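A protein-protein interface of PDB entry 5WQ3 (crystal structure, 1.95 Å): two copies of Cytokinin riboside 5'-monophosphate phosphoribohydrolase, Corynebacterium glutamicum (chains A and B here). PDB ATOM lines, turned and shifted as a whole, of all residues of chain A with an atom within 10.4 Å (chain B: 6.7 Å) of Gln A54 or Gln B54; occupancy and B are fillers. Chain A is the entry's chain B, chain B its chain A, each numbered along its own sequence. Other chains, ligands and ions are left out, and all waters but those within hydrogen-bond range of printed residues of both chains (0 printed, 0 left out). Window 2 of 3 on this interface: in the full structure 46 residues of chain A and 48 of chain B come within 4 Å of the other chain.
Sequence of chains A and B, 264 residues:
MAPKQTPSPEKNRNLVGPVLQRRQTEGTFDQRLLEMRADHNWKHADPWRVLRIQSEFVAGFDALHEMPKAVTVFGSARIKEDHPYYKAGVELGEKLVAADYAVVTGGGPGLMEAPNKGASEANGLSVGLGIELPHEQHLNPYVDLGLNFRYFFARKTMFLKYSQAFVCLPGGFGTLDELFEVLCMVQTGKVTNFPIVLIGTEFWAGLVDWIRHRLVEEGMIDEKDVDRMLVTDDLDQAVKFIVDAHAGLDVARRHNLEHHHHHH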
ATOM      1  N   ASP A  46      -7.153 -15.954   6.769  1.00  0.00           N
ATOM      2  CA  ASP A  46      -7.849 -16.769   7.693  1.00  0.00           C
ATOM      3  C   ASP A  46      -7.181 -18.018   8.225  1.00  0.00           C
ATOM      4  O   ASP A  46      -7.436 -18.349   9.382  1.00  0.00           O
ATOM      5  CB  ASP A  46      -9.205 -17.145   7.124  1.00  0.00           C
ATOM      6  CG  ASP A  46     -10.160 -15.920   6.984  1.00  0.00           C
ATOM      7  OD1 ASP A  46      -9.860 -14.822   7.459  1.00  0.00           O
ATOM      8  OD2 ASP A  46     -11.285 -16.090   6.435  1.00  0.00           O
ATOM      9  N   PRO A  47      -6.467 -18.780   7.405  1.00  0.00           N
ATOM     10  CA  PRO A  47      -5.884 -19.981   8.053  1.00  0.00           C
ATOM     11  C   PRO A  47      -4.978 -19.605   9.205  1.00  0.00           C
ATOM     12  O   PRO A  47      -5.044 -20.183  10.278  1.00  0.00           O
ATOM     13  CB  PRO A  47      -5.045 -20.642   6.941  1.00  0.00           C
ATOM     14  CG  PRO A  47      -5.706 -20.252   5.653  1.00  0.00           C
ATOM     15  CD  PRO A  47      -6.310 -18.827   5.930  1.00  0.00           C
ATOM     16  N   TRP A  48      -4.147 -18.627   8.971  1.00  0.00           N
ATOM     17  CA  TRP A  48      -3.213 -18.195   9.980  1.00  0.00           C
ATOM     18  C   TRP A  48      -3.936 -17.484  11.142  1.00  0.00           C
ATOM     19  O   TRP A  48      -3.589 -17.720  12.278  1.00  0.00           O
ATOM     20  CB  TRP A  48      -2.085 -17.397   9.413  1.00  0.00           C
ATOM     21  CG  TRP A  48      -0.988 -17.109  10.322  1.00  0.00           C
ATOM     22  CD1 TRP A  48      -0.649 -15.873  10.818  1.00  0.00           C
ATOM     23  CD2 TRP A  48       0.005 -18.029  10.840  1.00  0.00           C
ATOM     24  NE1 TRP A  48       0.474 -15.978  11.646  1.00  0.00           N
ATOM     25  CE2 TRP A  48       0.891 -17.283  11.665  1.00  0.00           C
ATOM     26  CE3 TRP A  48       0.184 -19.395  10.748  1.00  0.00           C
ATOM     27  CZ2 TRP A  48       1.972 -17.874  12.357  1.00  0.00           C
ATOM     28  CZ3 TRP A  48       1.272 -19.982  11.441  1.00  0.00           C
ATOM     29  CH2 TRP A  48       2.140 -19.220  12.236  1.00  0.00           C
ATOM     30  N   ARG A  49      -5.022 -16.753  10.883  1.00  0.00           N
ATOM     31  CA  ARG A  49      -5.733 -16.095  11.912  1.00  0.00           C
ATOM     32  C   ARG A  49      -6.268 -17.167  12.875  1.00  0.00           C
ATOM     33  O   ARG A  49      -6.167 -17.011  14.100  1.00  0.00           O
ATOM     34  CB  ARG A  49      -6.881 -15.187  11.308  1.00  0.00           C
ATOM     35  CG  ARG A  49      -7.658 -14.328  12.308  1.00  0.00           C
ATOM     36  CD  ARG A  49      -8.742 -13.440  11.639  1.00  0.00           C
ATOM     37  NE  ARG A  49      -8.167 -12.208  11.062  1.00  0.00           N
ATOM     38  CZ  ARG A  49      -7.796 -11.996   9.785  1.00  0.00           C
ATOM     39  NH1 ARG A  49      -7.272 -10.813   9.484  1.00  0.00           N
ATOM     40  NH2 ARG A  49      -7.924 -12.903   8.795  1.00  0.00           N
ATOM     41  N   VAL A  50      -6.824 -18.245  12.332  1.00  0.00           N
ATOM     42  CA  VAL A  50      -7.383 -19.336  13.108  1.00  0.00           C
ATOM     43  C   VAL A  50      -6.334 -20.027  13.985  1.00  0.00           C
ATOM     44  O   VAL A  50      -6.559 -20.238  15.159  1.00  0.00           O
ATOM     45  CB  VAL A  50      -8.127 -20.314  12.246  1.00  0.00           C
ATOM     46  CG1 VAL A  50      -8.583 -21.540  13.007  1.00  0.00           C
ATOM     47  CG2 VAL A  50      -9.369 -19.576  11.672  1.00  0.00           C
ATOM     48  N   LEU A  51      -5.200 -20.381  13.395  1.00  0.00           N
ATOM     49  CA  LEU A  51      -4.120 -20.969  14.185  1.00  0.00           C
ATOM     50  C   LEU A  51      -3.653 -20.001  15.324  1.00  0.00           C
ATOM     51  O   LEU A  51      -3.487 -20.454  16.483  1.00  0.00           O
ATOM     52  CB  LEU A  51      -2.992 -21.417  13.262  1.00  0.00           C
ATOM     53  CG  LEU A  51      -3.350 -22.476  12.214  1.00  0.00           C
ATOM     54  CD1 LEU A  51      -2.187 -22.627  11.223  1.00  0.00           C
ATOM     55  CD2 LEU A  51      -3.685 -23.824  12.819  1.00  0.00           C
ATOM     56  N   ARG A  52      -3.456 -18.706  15.020  1.00  0.00           N
ATOM     57  CA  ARG A  52      -3.128 -17.677  16.008  1.00  0.00           C
ATOM     58  C   ARG A  52      -4.159 -17.532  17.123  1.00  0.00           C
ATOM     59  O   ARG A  52      -3.812 -17.380  18.241  1.00  0.00           O
ATOM     60  CB  ARG A  52      -2.955 -16.271  15.404  1.00  0.00           C
ATOM     61  CG  ARG A  52      -1.689 -16.014  14.625  1.00  0.00           C
ATOM     62  CD  ARG A  52      -1.188 -14.558  14.666  1.00  0.00           C
ATOM     63  NE  ARG A  52      -2.029 -13.588  13.960  1.00  0.00           N
ATOM     64  CZ  ARG A  52      -1.599 -12.584  13.181  1.00  0.00           C
ATOM     65  NH1 ARG A  52      -2.489 -11.795  12.590  1.00  0.00           N
ATOM     66  NH2 ARG A  52      -0.310 -12.362  12.962  1.00  0.00           N
ATOM     67  N   ILE A  53      -5.428 -17.564  16.788  1.00  0.00           N
ATOM     68  CA  ILE A  53      -6.482 -17.556  17.775  1.00  0.00           C
ATOM     69  C   ILE A  53      -6.389 -18.759  18.644  1.00  0.00           C
ATOM     70  O   ILE A  53      -6.435 -18.615  19.856  1.00  0.00           O
ATOM     71  CB  ILE A  53      -7.906 -17.550  17.122  1.00  0.00           C
ATOM     72  CG1 ILE A  53      -8.171 -16.193  16.435  1.00  0.00           C
ATOM     73  CG2 ILE A  53      -8.961 -17.859  18.210  1.00  0.00           C
ATOM     74  CD1 ILE A  53      -9.431 -16.148  15.581  1.00  0.00           C
ATOM     75  N   GLN A  54      -6.246 -19.960  18.065  1.00  0.00           N
ATOM     76  CA  GLN A  54      -6.103 -21.137  18.868  1.00  0.00           C
ATOM     77  C   GLN A  54      -4.869 -20.990  19.801  1.00  0.00           C
ATOM     78  O   GLN A  54      -4.885 -21.382  20.975  1.00  0.00           O
ATOM     79  CB  GLN A  54      -5.913 -22.368  17.974  1.00  0.00           C
ATOM     80  CG  GLN A  54      -5.856 -23.674  18.750  1.00  0.00           C
ATOM     81  CD  GLN A  54      -5.800 -24.920  17.891  1.00  0.00           C
ATOM     82  OE1 GLN A  54      -6.800 -25.351  17.358  1.00  0.00           O
ATOM     83  NE2 GLN A  54      -4.670 -25.527  17.828  1.00  0.00           N
ATOM     84  N   SER A  55      -3.789 -20.456  19.251  1.00  0.00           N
ATOM     85  CA  SER A  55      -2.514 -20.426  19.990  1.00  0.00           C
ATOM     86  C   SER A  55      -2.747 -19.602  21.273  1.00  0.00           C
ATOM     87  O   SER A  55      -2.182 -19.910  22.331  1.00  0.00           O
ATOM     88  CB  SER A  55      -1.467 -19.669  19.155  1.00  0.00           C
ATOM     89  OG  SER A  55      -0.244 -19.603  19.853  1.00  0.00           O
ATOM     90  N   GLU A  56      -3.584 -18.551  21.130  1.00  0.00           N
ATOM     91  CA  GLU A  56      -3.845 -17.599  22.202  1.00  0.00           C
ATOM     92  C   GLU A  56      -4.743 -18.155  23.228  1.00  0.00           C
ATOM     93  O   GLU A  56      -4.486 -17.928  24.402  1.00  0.00           O
ATOM     94  CB  GLU A  56      -4.450 -16.271  21.720  1.00  0.00           C
ATOM     95  CG  GLU A  56      -3.393 -15.378  21.179  1.00  0.00           C
ATOM     96  CD  GLU A  56      -3.687 -13.890  21.297  1.00  0.00           C
ATOM     97  OE1 GLU A  56      -4.877 -13.400  21.347  1.00  0.00           O
ATOM     98  OE2 GLU A  56      -2.653 -13.217  21.275  1.00  0.00           O
ATOM     99  N   PHE A  57      -5.835 -18.816  22.822  1.00  0.00           N
ATOM    100  CA  PHE A  57      -6.601 -19.548  23.807  1.00  0.00           C
ATOM    101  C   PHE A  57      -5.775 -20.588  24.544  1.00  0.00           C
ATOM    102  O   PHE A  57      -5.943 -20.776  25.726  1.00  0.00           O
ATOM    103  CB  PHE A  57      -7.883 -20.148  23.264  1.00  0.00           C
ATOM    104  CG  PHE A  57      -8.943 -19.120  23.040  1.00  0.00           C
ATOM    105  CD1 PHE A  57      -9.782 -18.738  24.054  1.00  0.00           C
ATOM    106  CD2 PHE A  57      -9.020 -18.479  21.860  1.00  0.00           C
ATOM    107  CE1 PHE A  57     -10.737 -17.729  23.881  1.00  0.00           C
ATOM    108  CE2 PHE A  57      -9.967 -17.466  21.661  1.00  0.00           C
ATOM    109  CZ  PHE A  57     -10.841 -17.108  22.684  1.00  0.00           C
ATOM    110  N   VAL A  58      -5.000 -21.373  23.837  1.00  0.00           N
ATOM    111  CA  VAL A  58      -4.260 -22.421  24.491  1.00  0.00           C
ATOM    112  C   VAL A  58      -3.354 -21.768  25.541  1.00  0.00           C
ATOM    113  O   VAL A  58      -3.254 -22.249  26.675  1.00  0.00           O
ATOM    114  CB  VAL A  58      -3.449 -23.253  23.502  1.00  0.00           C
ATOM    115  CG1 VAL A  58      -2.402 -24.138  24.207  1.00  0.00           C
ATOM    116  CG2 VAL A  58      -4.352 -24.086  22.675  1.00  0.00           C
ATOM    117  N   ALA A  59      -2.669 -20.709  25.164  1.00  0.00           N
ATOM    118  CA  ALA A  59      -1.614 -20.133  26.072  1.00  0.00           C
ATOM    119  C   ALA A  59      -2.273 -19.528  27.330  1.00  0.00           C
ATOM    120  O   ALA A  59      -1.761 -19.669  28.437  1.00  0.00           O
ATOM    121  CB  ALA A  59      -0.785 -19.097  25.364  1.00  0.00           C
ATOM    122  N   GLY A  60      -3.478 -18.943  27.164  1.00  0.00           N
ATOM    123  CA  GLY A  60      -4.181 -18.404  28.285  1.00  0.00           C
ATOM    124  C   GLY A  60      -4.783 -19.483  29.160  1.00  0.00           C
ATOM    125  O   GLY A  60      -4.616 -19.411  30.390  1.00  0.00           O
ATOM    126  N   PHE A  61      -5.497 -20.468  28.583  1.00  0.00           N
ATOM    127  CA  PHE A  61      -5.979 -21.598  29.387  1.00  0.00           C
ATOM    128  C   PHE A  61      -4.861 -22.339  30.126  1.00  0.00           C
ATOM    129  O   PHE A  61      -5.075 -22.773  31.256  1.00  0.00           O
ATOM    130  CB  PHE A  61      -6.737 -22.622  28.622  1.00  0.00           C
ATOM    131  CG  PHE A  61      -7.990 -22.088  27.945  1.00  0.00           C
ATOM    132  CD1 PHE A  61      -8.538 -20.866  28.264  1.00  0.00           C
ATOM    133  CD2 PHE A  61      -8.595 -22.843  26.978  1.00  0.00           C
ATOM    134  CE1 PHE A  61      -9.709 -20.434  27.643  1.00  0.00           C
ATOM    135  CE2 PHE A  61      -9.749 -22.404  26.341  1.00  0.00           C
ATOM    136  CZ  PHE A  61     -10.294 -21.197  26.667  1.00  0.00           C
ATOM    137  N   ASP A  62      -3.676 -22.416  29.519  1.00  0.00           N
ATOM    138  CA  ASP A  62      -2.598 -23.105  30.197  1.00  0.00           C
ATOM    139  C   ASP A  62      -2.089 -22.295  31.387  1.00  0.00           C
ATOM    140  O   ASP A  62      -1.977 -22.836  32.452  1.00  0.00           O
ATOM    141  CB  ASP A  62      -1.487 -23.425  29.270  1.00  0.00           C
ATOM    142  CG  ASP A  62      -0.560 -24.425  29.837  1.00  0.00           C
ATOM    143  OD1 ASP A  62      -0.887 -25.635  29.833  1.00  0.00           O
ATOM    144  OD2 ASP A  62       0.514 -23.975  30.268  1.00  0.00           O
ATOM    145  N   PHE A 149      -1.755 -10.670  24.655  1.00  0.00           N
ATOM    146  CA  PHE A 149      -2.684 -11.151  23.655  1.00  0.00           C
ATOM    147  C   PHE A 149      -2.624 -10.231  22.428  1.00  0.00           C
ATOM    148  O   PHE A 149      -2.467  -9.018  22.582  1.00  0.00           O
ATOM    149  CB  PHE A 149      -4.076 -11.114  24.234  1.00  0.00           C
ATOM    150  CG  PHE A 149      -4.315 -12.174  25.268  1.00  0.00           C
ATOM    151  CD1 PHE A 149      -3.987 -11.967  26.562  1.00  0.00           C
ATOM    152  CD2 PHE A 149      -4.874 -13.387  24.921  1.00  0.00           C
ATOM    153  CE1 PHE A 149      -4.191 -12.915  27.522  1.00  0.00           C
ATOM    154  CE2 PHE A 149      -5.070 -14.364  25.888  1.00  0.00           C
ATOM    155  CZ  PHE A 149      -4.719 -14.121  27.203  1.00  0.00           C
ATOM    156  N   ARG A 150      -2.758 -10.786  21.232  1.00  0.00           N
ATOM    157  CA  ARG A 150      -2.973  -9.981  20.062  1.00  0.00           C
ATOM    158  C   ARG A 150      -4.429  -9.792  19.833  1.00  0.00           C
ATOM    159  O   ARG A 150      -4.816  -8.813  19.228  1.00  0.00           O
ATOM    160  CB  ARG A 150      -2.389 -10.674  18.830  1.00  0.00           C
ATOM    161  CG  ARG A 150      -2.540  -9.932  17.499  1.00  0.00           C
ATOM    162  CD  ARG A 150      -2.012 -10.849  16.379  1.00  0.00           C
ATOM    163  NE  ARG A 150      -1.337 -10.142  15.278  1.00  0.00           N
ATOM    164  CZ  ARG A 150      -0.078  -9.694  15.296  1.00  0.00           C
ATOM    165  NH1 ARG A 150       0.420  -9.075  14.226  1.00  0.00           N
ATOM    166  NH2 ARG A 150       0.688  -9.833  16.371  1.00  0.00           N
ATOM    167  N   TYR A 151      -5.250 -10.750  20.212  1.00  0.00           N
ATOM    168  CA  TYR A 151      -6.690 -10.638  19.863  1.00  0.00           C
ATOM    169  C   TYR A 151      -7.482 -10.127  21.050  1.00  0.00           C
ATOM    170  O   TYR A 151      -7.662 -10.802  22.056  1.00  0.00           O
ATOM    171  CB  TYR A 151      -7.250 -11.987  19.430  1.00  0.00           C
ATOM    172  CG  TYR A 151      -6.685 -12.379  18.100  1.00  0.00           C
ATOM    173  CD1 TYR A 151      -7.071 -11.689  16.922  1.00  0.00           C
ATOM    174  CD2 TYR A 151      -5.723 -13.351  18.002  1.00  0.00           C
ATOM    175  CE1 TYR A 151      -6.541 -12.012  15.702  1.00  0.00           C
ATOM    176  CE2 TYR A 151      -5.174 -13.676  16.782  1.00  0.00           C
ATOM    177  CZ  TYR A 151      -5.583 -13.002  15.642  1.00  0.00           C
ATOM    178  OH  TYR A 151      -5.020 -13.334  14.432  1.00  0.00           O
ATOM    179  N   ALA A 154     -10.107 -12.556  22.514  1.00  0.00           N
ATOM    180  CA  ALA A 154      -9.534 -13.583  23.334  1.00  0.00           C
ATOM    181  C   ALA A 154      -9.203 -13.100  24.751  1.00  0.00           C
ATOM    182  O   ALA A 154      -9.495 -13.757  25.706  1.00  0.00           O
ATOM    183  CB  ALA A 154      -8.296 -14.132  22.672  1.00  0.00           C
ATOM    184  N   MET A 158     -10.916 -14.194  28.727  1.00  0.00           N
ATOM    185  CA  MET A 158     -10.175 -14.651  29.856  1.00  0.00           C
ATOM    186  C   MET A 158     -10.606 -13.861  31.129  1.00  0.00           C
ATOM    187  O   MET A 158     -10.626 -14.433  32.201  1.00  0.00           O
ATOM    188  CB  MET A 158      -8.686 -14.416  29.653  1.00  0.00           C
ATOM    189  CG  MET A 158      -8.081 -15.133  28.476  1.00  0.00           C
ATOM    190  SD  MET A 158      -8.059 -16.906  28.591  1.00  0.00           S
ATOM    191  CE  MET A 158      -7.893 -17.211  26.841  1.00  0.00           C
ATOM    192  N   ARG B  49     -12.583 -27.811  24.290  1.00  0.00           N
ATOM    193  CA  ARG B  49     -13.023 -26.440  24.181  1.00  0.00           C
ATOM    194  C   ARG B  49     -12.278 -25.636  23.129  1.00  0.00           C
ATOM    195  O   ARG B  49     -12.850 -24.962  22.378  1.00  0.00           O
ATOM    196  CB  ARG B  49     -12.927 -25.738  25.524  1.00  0.00           C
ATOM    197  CG  ARG B  49     -13.590 -24.373  25.544  1.00  0.00           C
ATOM    198  CD  ARG B  49     -14.253 -24.045  26.873  1.00  0.00           C
ATOM    199  NE  ARG B  49     -13.562 -24.642  28.008  1.00  0.00           N
ATOM    200  CZ  ARG B  49     -14.113 -25.400  28.941  1.00  0.00           C
ATOM    201  NH1 ARG B  49     -15.402 -25.692  28.932  1.00  0.00           N
ATOM    202  NH2 ARG B  49     -13.357 -25.872  29.894  1.00  0.00           N
ATOM    203  N   VAL B  50     -10.971 -25.730  23.139  1.00  0.00           N
ATOM    204  CA  VAL B  50     -10.137 -25.068  22.183  1.00  0.00           C
ATOM    205  C   VAL B  50     -10.520 -25.524  20.761  1.00  0.00           C
ATOM    206  O   VAL B  50     -10.685 -24.737  19.899  1.00  0.00           O
ATOM    207  CB  VAL B  50      -8.651 -25.299  22.501  1.00  0.00           C
ATOM    208  CG1 VAL B  50      -7.780 -24.956  21.330  1.00  0.00           C
ATOM    209  CG2 VAL B  50      -8.279 -24.489  23.714  1.00  0.00           C
ATOM    210  N   LEU B  51     -10.681 -26.822  20.585  1.00  0.00           N
ATOM    211  CA  LEU B  51     -11.129 -27.392  19.322  1.00  0.00           C
ATOM    212  C   LEU B  51     -12.518 -26.894  18.882  1.00  0.00           C
ATOM    213  O   LEU B  51     -12.721 -26.611  17.767  1.00  0.00           O
ATOM    214  CB  LEU B  51     -11.099 -28.895  19.389  1.00  0.00           C
ATOM    215  CG  LEU B  51      -9.710 -29.501  19.578  1.00  0.00           C
ATOM    216  CD1 LEU B  51      -9.778 -30.997  19.571  1.00  0.00           C
ATOM    217  CD2 LEU B  51      -8.760 -28.966  18.548  1.00  0.00           C
ATOM    218  N   ARG B  52     -13.425 -26.807  19.815  1.00  0.00           N
ATOM    219  CA  ARG B  52     -14.734 -26.271  19.539  1.00  0.00           C
ATOM    220  C   ARG B  52     -14.687 -24.804  19.178  1.00  0.00           C
ATOM    221  O   ARG B  52     -15.403 -24.367  18.327  1.00  0.00           O
ATOM    222  CB  ARG B  52     -15.639 -26.434  20.734  1.00  0.00           C
ATOM    223  CG  ARG B  52     -16.160 -27.807  20.913  1.00  0.00           C
ATOM    224  CD  ARG B  52     -17.157 -27.773  22.010  1.00  0.00           C
ATOM    225  NE  ARG B  52     -18.419 -27.276  21.524  1.00  0.00           N
ATOM    226  CZ  ARG B  52     -19.473 -27.112  22.304  1.00  0.00           C
ATOM    227  NH1 ARG B  52     -19.364 -27.427  23.576  1.00  0.00           N
ATOM    228  NH2 ARG B  52     -20.622 -26.685  21.808  1.00  0.00           N
ATOM    229  N   ILE B  53     -13.823 -24.068  19.835  1.00  0.00           N
ATOM    230  CA  ILE B  53     -13.721 -22.651  19.591  1.00  0.00           C
ATOM    231  C   ILE B  53     -13.267 -22.511  18.173  1.00  0.00           C
ATOM    232  O   ILE B  53     -13.848 -21.819  17.420  1.00  0.00           O
ATOM    233  CB  ILE B  53     -12.769 -21.921  20.571  1.00  0.00           C
ATOM    234  CG1 ILE B  53     -13.444 -21.736  21.930  1.00  0.00           C
ATOM    235  CG2 ILE B  53     -12.341 -20.573  20.033  1.00  0.00           C
ATOM    236  CD1 ILE B  53     -12.500 -21.478  23.072  1.00  0.00           C
ATOM    237  N   GLN B  54     -12.184 -23.174  17.857  1.00  0.00           N
ATOM    238  CA  GLN B  54     -11.662 -23.175  16.525  1.00  0.00           C
ATOM    239  C   GLN B  54     -12.725 -23.523  15.508  1.00  0.00           C
ATOM    240  O   GLN B  54     -12.824 -22.910  14.491  1.00  0.00           O
ATOM    241  CB  GLN B  54     -10.535 -24.186  16.422  1.00  0.00           C
ATOM    242  CG  GLN B  54     -10.085 -24.462  15.021  1.00  0.00           C
ATOM    243  CD  GLN B  54      -8.668 -24.871  14.947  1.00  0.00           C
ATOM    244  OE1 GLN B  54      -7.828 -24.178  15.423  1.00  0.00           O
ATOM    245  NE2 GLN B  54      -8.404 -25.963  14.343  1.00  0.00           N
ATOM    246  N   SER B  55     -13.433 -24.591  15.770  1.00  0.00           N
ATOM    247  CA  SER B  55     -14.380 -25.069  14.815  1.00  0.00           C
ATOM    248  C   SER B  55     -15.375 -23.964  14.481  1.00  0.00           C
ATOM    249  O   SER B  55     -15.811 -23.864  13.375  1.00  0.00           O
ATOM    250  CB  SER B  55     -15.040 -26.338  15.262  1.00  0.00           C
ATOM    251  OG  SER B  55     -16.171 -26.062  15.989  1.00  0.00           O
ATOM    252  N   GLU B  56     -15.701 -23.140  15.464  1.00  0.00           N
ATOM    253  CA  GLU B  56     -16.700 -22.080  15.289  1.00  0.00           C
ATOM    254  C   GLU B  56     -16.170 -20.900  14.503  1.00  0.00           C
ATOM    255  O   GLU B  56     -16.833 -20.385  13.579  1.00  0.00           O
ATOM    256  CB  GLU B  56     -17.293 -21.674  16.650  1.00  0.00           C
ATOM    257  CG  GLU B  56     -18.329 -20.587  16.521  1.00  0.00           C
ATOM    258  CD  GLU B  56     -19.340 -20.566  17.657  1.00  0.00           C
ATOM    259  OE1 GLU B  56     -19.321 -19.552  18.356  1.00  0.00           O
ATOM    260  OE2 GLU B  56     -20.165 -21.508  17.835  1.00  0.00           O
ATOM    261  N   PHE B  57     -14.925 -20.511  14.779  1.00  0.00           N
ATOM    262  CA  PHE B  57     -14.257 -19.551  13.904  1.00  0.00           C
ATOM    263  C   PHE B  57     -14.133 -20.015  12.439  1.00  0.00           C
ATOM    264  O   PHE B  57     -14.404 -19.233  11.558  1.00  0.00           O
ATOM    265  CB  PHE B  57     -12.908 -19.085  14.458  1.00  0.00           C
ATOM    266  CG  PHE B  57     -13.019 -18.084  15.584  1.00  0.00           C
ATOM    267  CD1 PHE B  57     -13.284 -16.742  15.325  1.00  0.00           C
ATOM    268  CD2 PHE B  57     -12.818 -18.447  16.918  1.00  0.00           C
ATOM    269  CE1 PHE B  57     -13.311 -15.802  16.394  1.00  0.00           C
ATOM    270  CE2 PHE B  57     -12.901 -17.519  17.972  1.00  0.00           C
ATOM    271  CZ  PHE B  57     -13.097 -16.190  17.712  1.00  0.00           C
ATOM    272  N   VAL B  58     -13.751 -21.292  12.194  1.00  0.00           N
ATOM    273  CA  VAL B  58     -13.608 -21.800  10.843  1.00  0.00           C
ATOM    274  C   VAL B  58     -15.021 -21.683  10.150  1.00  0.00           C
ATOM    275  O   VAL B  58     -15.155 -21.150   9.054  1.00  0.00           O
ATOM    276  CB  VAL B  58     -13.101 -23.230  10.813  1.00  0.00           C
ATOM    277  CG1 VAL B  58     -13.238 -23.826   9.392  1.00  0.00           C
ATOM    278  CG2 VAL B  58     -11.595 -23.218  11.275  1.00  0.00           C
ATOM    279  N   ALA B  59     -16.021 -22.169  10.820  1.00  0.00           N
ATOM    280  CA  ALA B  59     -17.363 -22.131  10.233  1.00  0.00           C
ATOM    281  C   ALA B  59     -17.840 -20.756   9.917  1.00  0.00           C
ATOM    282  O   ALA B  59     -18.506 -20.532   8.884  1.00  0.00           O
ATOM    283  CB  ALA B  59     -18.354 -22.793  11.141  1.00  0.00           C
ATOM    284  N   TYR B 151     -20.351 -19.216  20.829  1.00  0.00           N
ATOM    285  CA  TYR B 151     -19.423 -18.348  21.591  1.00  0.00           C
ATOM    286  C   TYR B 151     -19.657 -16.854  21.291  1.00  0.00           C
ATOM    287  O   TYR B 151     -19.496 -16.404  20.187  1.00  0.00           O
ATOM    288  CB  TYR B 151     -17.967 -18.733  21.334  1.00  0.00           C
ATOM    289  CG  TYR B 151     -17.703 -20.148  21.771  1.00  0.00           C
ATOM    290  CD1 TYR B 151     -17.678 -20.483  23.125  1.00  0.00           C
ATOM    291  CD2 TYR B 151     -17.500 -21.142  20.833  1.00  0.00           C
ATOM    292  CE1 TYR B 151     -17.480 -21.795  23.534  1.00  0.00           C
ATOM    293  CE2 TYR B 151     -17.298 -22.433  21.196  1.00  0.00           C
ATOM    294  CZ  TYR B 151     -17.263 -22.774  22.541  1.00  0.00           C
ATOM    295  OH  TYR B 151     -17.059 -24.099  22.843  1.00  0.00           O
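OE1 of Gln A54 sits close to OE1 of Gln B54 (2.5 Å).
Among the printed residues, pairs that only touch across the chains: Val A50 with Gln B54 (3.7 Å), Val A50 with Val B58 (3.9 Å), Ile A53 with Phe B57 (3.9 Å), Gln A54 with Val B50 (3.5 Å), Phe A57 with Ile B53 (3.98 Å), Val A58 with Val B50 (3.8 Å) and Phe A61 with Val B50 (3.7 Å).
Printed residues of chain B within 4 Å of Val A50: Gln B54 (3.7 Å) and Val B58 (3.9 Å). Of the printed residues of chain B, Ile A53 touches Phe B57 (3.9 Å). Of chain B, only Val B50 and Gln B54 come within 4 Å of Gln A54. Ala A59 touches none of the printed residues of chain B. Of the printed residues of chain B, Phe A61 touches Val B50. Asp A62 touches none of the printed residues of chain B. Of the printed residues of chain A, Ile B53 touches Phe A57 (3.98 Å). Printed residues of chain A within 4 Å of Gln B54: Val A50 and Gln A54. Of the printed residues of chain A, Phe B57 touches Ile A53. The nearest residue of chain B that does not touch Gln A54 is Leu B51 (4.3 Å). The nearest printed residue of chain A that does not touch Phe B57 is Val A50 (4.5 Å).
Of the 12 printed residues of chain B, 5 touch a printed residue of chain A. Hydrophobic or aromatic side chains of chain B within 4 Å of the printed part of chain A: Val B50, Ile B53, Phe B57 and Val B58. Along chain B the printed residues that touch a printed residue of chain A span positions 50 to 58. Printed residues of chain A that touch a printed residue of chain B: Val A50, Ile A53, Gln A54, Phe A57, Val A58 and Phe A61. Hydrophobic or aromatic side chains of chain A within 4 Å of the printed part of chain B: Val A50, Ile A53, Phe A57, Val A58 and Phe A61. Along chain A the printed residues that touch a printed residue of chain B span positions 50 to 61. Among the printed residues, no Asp or Glu carboxylate lies within 4 Å of a Lys or Arg side-chain nitrogen of the other chain.
Val A50 touches Gln B54, and with the chains exchanged Gln A54 touches Val B50. Val A50 touches Val B58, and with the chains exchanged Val A58 touches Val B50. Ile A53 touches Phe B57, and with the chains exchanged Phe A57 touches Ile B53. Gln A54 touches its own counterpart, Gln B54. Positions printed for both chains: 49, 50, 51, 52, 53, 54, 55, 56, 57, 58, 59 and 151. Of the 8 pairs that touch across the chains among the printed residues, 7 have their exchanged pair printed and touching as well.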
